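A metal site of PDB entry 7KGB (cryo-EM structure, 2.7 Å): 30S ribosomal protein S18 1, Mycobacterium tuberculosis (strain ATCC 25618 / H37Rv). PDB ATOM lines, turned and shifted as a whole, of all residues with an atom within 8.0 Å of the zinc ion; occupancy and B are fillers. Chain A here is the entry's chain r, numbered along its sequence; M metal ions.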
ATOM      1  N   CYS A  20      -4.438  -6.324 -26.427  1.00  0.00           N
ATOM      2  CA  CYS A  20      -3.749  -7.247 -25.546  1.00  0.00           C
ATOM      3  C   CYS A  20      -4.657  -8.411 -25.171  1.00  0.00           C
ATOM      4  O   CYS A  20      -5.695  -8.214 -24.556  1.00  0.00           O
ATOM      5  CB  CYS A  20      -3.261  -6.537 -24.278  1.00  0.00           C
ATOM      6  SG  CYS A  20      -2.104  -7.503 -23.297  1.00  0.00           S
ATOM      7  N   VAL A  21      -4.247  -9.620 -25.547  1.00  0.00           N
ATOM      8  CA  VAL A  21      -5.081 -10.790 -25.298  1.00  0.00           C
ATOM      9  C   VAL A  21      -5.212 -11.071 -23.811  1.00  0.00           C
ATOM     10  O   VAL A  21      -6.295 -11.415 -23.323  1.00  0.00           O
ATOM     11  CB  VAL A  21      -4.516 -12.010 -26.059  1.00  0.00           C
ATOM     12  CG1 VAL A  21      -5.294 -13.261 -25.696  1.00  0.00           C
ATOM     13  CG2 VAL A  21      -4.580 -11.766 -27.539  1.00  0.00           C
ATOM     14  N   PHE A  22      -4.116 -10.940 -23.071  1.00  0.00           N
ATOM     15  CA  PHE A  22      -4.149 -11.298 -21.658  1.00  0.00           C
ATOM     16  C   PHE A  22      -4.920 -10.280 -20.831  1.00  0.00           C
ATOM     17  O   PHE A  22      -5.452 -10.622 -19.771  1.00  0.00           O
ATOM     18  CB  PHE A  22      -2.722 -11.458 -21.135  1.00  0.00           C
ATOM     19  CG  PHE A  22      -1.825 -12.210 -22.064  1.00  0.00           C
ATOM     20  CD1 PHE A  22      -1.889 -13.592 -22.133  1.00  0.00           C
ATOM     21  CD2 PHE A  22      -0.926 -11.558 -22.869  1.00  0.00           C
ATOM     22  CE1 PHE A  22      -1.079 -14.296 -22.985  1.00  0.00           C
ATOM     23  CE2 PHE A  22      -0.110 -12.249 -23.720  1.00  0.00           C
ATOM     24  CZ  PHE A  22      -0.179 -13.622 -23.781  1.00  0.00           C
ATOM     25  N   CYS A  23      -4.973  -9.033 -21.287  1.00  0.00           N
ATOM     26  CA  CYS A  23      -5.881  -8.086 -20.654  1.00  0.00           C
ATOM     27  C   CYS A  23      -7.321  -8.329 -21.089  1.00  0.00           C
ATOM     28  O   CYS A  23      -8.242  -8.216 -20.284  1.00  0.00           O
ATOM     29  CB  CYS A  23      -5.465  -6.654 -20.976  1.00  0.00           C
ATOM     30  SG  CYS A  23      -3.971  -6.102 -20.147  1.00  0.00           S
ATOM     31  N   ALA A  24      -7.514  -8.656 -22.374  1.00  0.00           N
ATOM     32  CA  ALA A  24      -8.855  -8.841 -22.902  1.00  0.00           C
ATOM     33  C   ALA A  24      -9.573  -9.967 -22.182  1.00  0.00           C
ATOM     34  O   ALA A  24     -10.700  -9.797 -21.701  1.00  0.00           O
ATOM     35  CB  ALA A  24      -8.792  -9.111 -24.406  1.00  0.00           C
ATOM     36  N   LYS A  25      -8.933 -11.119 -22.082  1.00  0.00           N
ATOM     37  CA  LYS A  25      -9.462 -12.232 -21.306  1.00  0.00           C
ATOM     38  C   LYS A  25      -8.502 -12.506 -20.167  1.00  0.00           C
ATOM     39  O   LYS A  25      -7.322 -12.811 -20.387  1.00  0.00           O
ATOM     40  CB  LYS A  25      -9.687 -13.469 -22.180  1.00  0.00           C
ATOM     41  CG  LYS A  25      -8.453 -14.047 -22.852  1.00  0.00           C
ATOM     42  CD  LYS A  25      -8.827 -15.232 -23.716  1.00  0.00           C
ATOM     43  CE  LYS A  25      -9.383 -16.375 -22.872  1.00  0.00           C
ATOM     44  NZ  LYS A  25      -8.364 -16.951 -21.965  1.00  0.00           N
ATOM     45  N   ILE A  30       0.105 -17.206 -17.835  1.00  0.00           N
ATOM     46  CA  ILE A  30       1.336 -17.325 -18.613  1.00  0.00           C
ATOM     47  C   ILE A  30       2.347 -18.083 -17.778  1.00  0.00           C
ATOM     48  O   ILE A  30       2.635 -17.709 -16.648  1.00  0.00           O
ATOM     49  CB  ILE A  30       1.885 -15.948 -19.012  1.00  0.00           C
ATOM     50  CG1 ILE A  30       0.907 -15.211 -19.910  1.00  0.00           C
ATOM     51  CG2 ILE A  30       3.211 -16.103 -19.723  1.00  0.00           C
ATOM     52  CD1 ILE A  30       1.261 -13.769 -20.114  1.00  0.00           C
ATOM     53  N   GLY A  55       0.912  -6.360 -29.655  1.00  0.00           N
ATOM     54  CA  GLY A  55      -0.103  -5.607 -28.972  1.00  0.00           C
ATOM     55  C   GLY A  55      -0.215  -5.874 -27.492  1.00  0.00           C
ATOM     56  O   GLY A  55      -1.176  -5.399 -26.868  1.00  0.00           O
ATOM     57  N   ASN A  56       0.710  -6.623 -26.916  1.00  0.00           N
ATOM     58  CA  ASN A  56       0.690  -6.846 -25.479  1.00  0.00           C
ATOM     59  C   ASN A  56       0.978  -5.556 -24.727  1.00  0.00           C
ATOM     60  O   ASN A  56       1.682  -4.665 -25.226  1.00  0.00           O
ATOM     61  CB  ASN A  56       1.718  -7.899 -25.092  1.00  0.00           C
ATOM     62  CG  ASN A  56       1.417  -9.246 -25.699  1.00  0.00           C
ATOM     63  OD1 ASN A  56       0.447  -9.392 -26.447  1.00  0.00           O
ATOM     64  ND2 ASN A  56       2.234 -10.236 -25.380  1.00  0.00           N
ATOM     65  N   CYS A  57       0.433  -5.448 -23.527  1.00  0.00           N
ATOM     66  CA  CYS A  57       0.806  -4.366 -22.646  1.00  0.00           C
ATOM     67  C   CYS A  57       2.228  -4.593 -22.139  1.00  0.00           C
ATOM     68  O   CYS A  57       2.843  -5.626 -22.395  1.00  0.00           O
ATOM     69  CB  CYS A  57      -0.163  -4.256 -21.481  1.00  0.00           C
ATOM     70  SG  CYS A  57      -0.210  -5.721 -20.444  1.00  0.00           S
ATOM     71  N   VAL A  58       2.746  -3.616 -21.410  1.00  0.00           N
ATOM     72  CA  VAL A  58       4.120  -3.714 -20.935  1.00  0.00           C
ATOM     73  C   VAL A  58       4.275  -4.873 -19.964  1.00  0.00           C
ATOM     74  O   VAL A  58       5.239  -5.647 -20.048  1.00  0.00           O
ATOM     75  CB  VAL A  58       4.549  -2.378 -20.306  1.00  0.00           C
ATOM     76  CG1 VAL A  58       6.043  -2.364 -20.100  1.00  0.00           C
ATOM     77  CG2 VAL A  58       4.133  -1.234 -21.198  1.00  0.00           C
ATOM     78  N   GLN A  59       3.338  -5.021 -19.030  1.00  0.00           N
ATOM     79  CA  GLN A  59       3.484  -6.059 -18.008  1.00  0.00           C
ATOM     80  C   GLN A  59       3.357  -7.446 -18.609  1.00  0.00           C
ATOM     81  O   GLN A  59       4.141  -8.349 -18.274  1.00  0.00           O
ATOM     82  CB  GLN A  59       2.442  -5.845 -16.920  1.00  0.00           C
ATOM     83  CG  GLN A  59       2.388  -4.424 -16.428  1.00  0.00           C
ATOM     84  CD  GLN A  59       1.409  -4.228 -15.303  1.00  0.00           C
ATOM     85  OE1 GLN A  59       1.075  -5.175 -14.593  1.00  0.00           O
ATOM     86  NE2 GLN A  59       0.953  -3.010 -15.124  1.00  0.00           N
ATOM     87  N   HIS A  60       2.412  -7.651 -19.522  1.00  0.00           N
ATOM     88  CA  HIS A  60       2.274  -8.969 -20.131  1.00  0.00           C
ATOM     89  C   HIS A  60       3.390  -9.250 -21.113  1.00  0.00           C
ATOM     90  O   HIS A  60       3.781 -10.404 -21.292  1.00  0.00           O
ATOM     91  CB  HIS A  60       0.909  -9.095 -20.784  1.00  0.00           C
ATOM     92  CG  HIS A  60      -0.202  -9.182 -19.794  1.00  0.00           C
ATOM     93  ND1 HIS A  60      -1.235  -8.277 -19.747  1.00  0.00           N
ATOM     94  CD2 HIS A  60      -0.439 -10.066 -18.796  1.00  0.00           C
ATOM     95  CE1 HIS A  60      -2.061  -8.594 -18.762  1.00  0.00           C
ATOM     96  NE2 HIS A  60      -1.598  -9.674 -18.174  1.00  0.00           N
ATOM     97  N   GLN A  61       3.936  -8.215 -21.745  1.00  0.00           N
ATOM     98  CA  GLN A  61       5.133  -8.403 -22.559  1.00  0.00           C
ATOM     99  C   GLN A  61       6.299  -8.868 -21.706  1.00  0.00           C
ATOM    100  O   GLN A  61       7.053  -9.774 -22.102  1.00  0.00           O
ATOM    101  CB  GLN A  61       5.485  -7.116 -23.289  1.00  0.00           C
ATOM    102  CG  GLN A  61       6.785  -7.191 -24.054  1.00  0.00           C
ATOM    103  CD  GLN A  61       6.616  -7.837 -25.402  1.00  0.00           C
ATOM    104  OE1 GLN A  61       5.501  -7.970 -25.909  1.00  0.00           O
ATOM    105  NE2 GLN A  61       7.714  -8.255 -25.996  1.00  0.00           N
ATOM    106  N   ASP A  63       6.020 -10.539 -18.893  1.00  0.00           N
ATOM    107  CA  ASP A  63       5.702 -11.912 -18.520  1.00  0.00           C
ATOM    108  C   ASP A  63       6.018 -12.892 -19.640  1.00  0.00           C
ATOM    109  O   ASP A  63       6.566 -13.965 -19.393  1.00  0.00           O
ATOM    110  CB  ASP A  63       4.225 -12.021 -18.127  1.00  0.00           C
ATOM    111  CG  ASP A  63       3.882 -11.223 -16.897  1.00  0.00           C
ATOM    112  OD1 ASP A  63       2.729 -10.758 -16.796  1.00  0.00           O
ATOM    113  OD2 ASP A  63       4.765 -11.055 -16.038  1.00  0.00           O
HETATM  114 ZN    ZN M   1      -2.038  -6.996 -21.045  1.00  0.00          ZN
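The zinc ion is bound by a ring nitrogen (ND1) of His 60 (2.0 Å), the side-chain sulfur (SG) of Cys 57 (2.3 Å), the side-chain sulfur (SG) of Cys 20 (2.3 Å) and the side-chain sulfur (SG) of Cys 23 (2.3 Å). The zinc ion has four donor atoms within binding distance.
Of the 15 residues printed, 4 come within 4 Å of the zinc ion. The nearest printed residue that does not touch the zinc ion is Phe 22 (4.4 Å).
The backbone carbonyl oxygen (O) of Gly 55 sits at hydrogen-bond distance from the backbone NH (N) of Cys 20.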
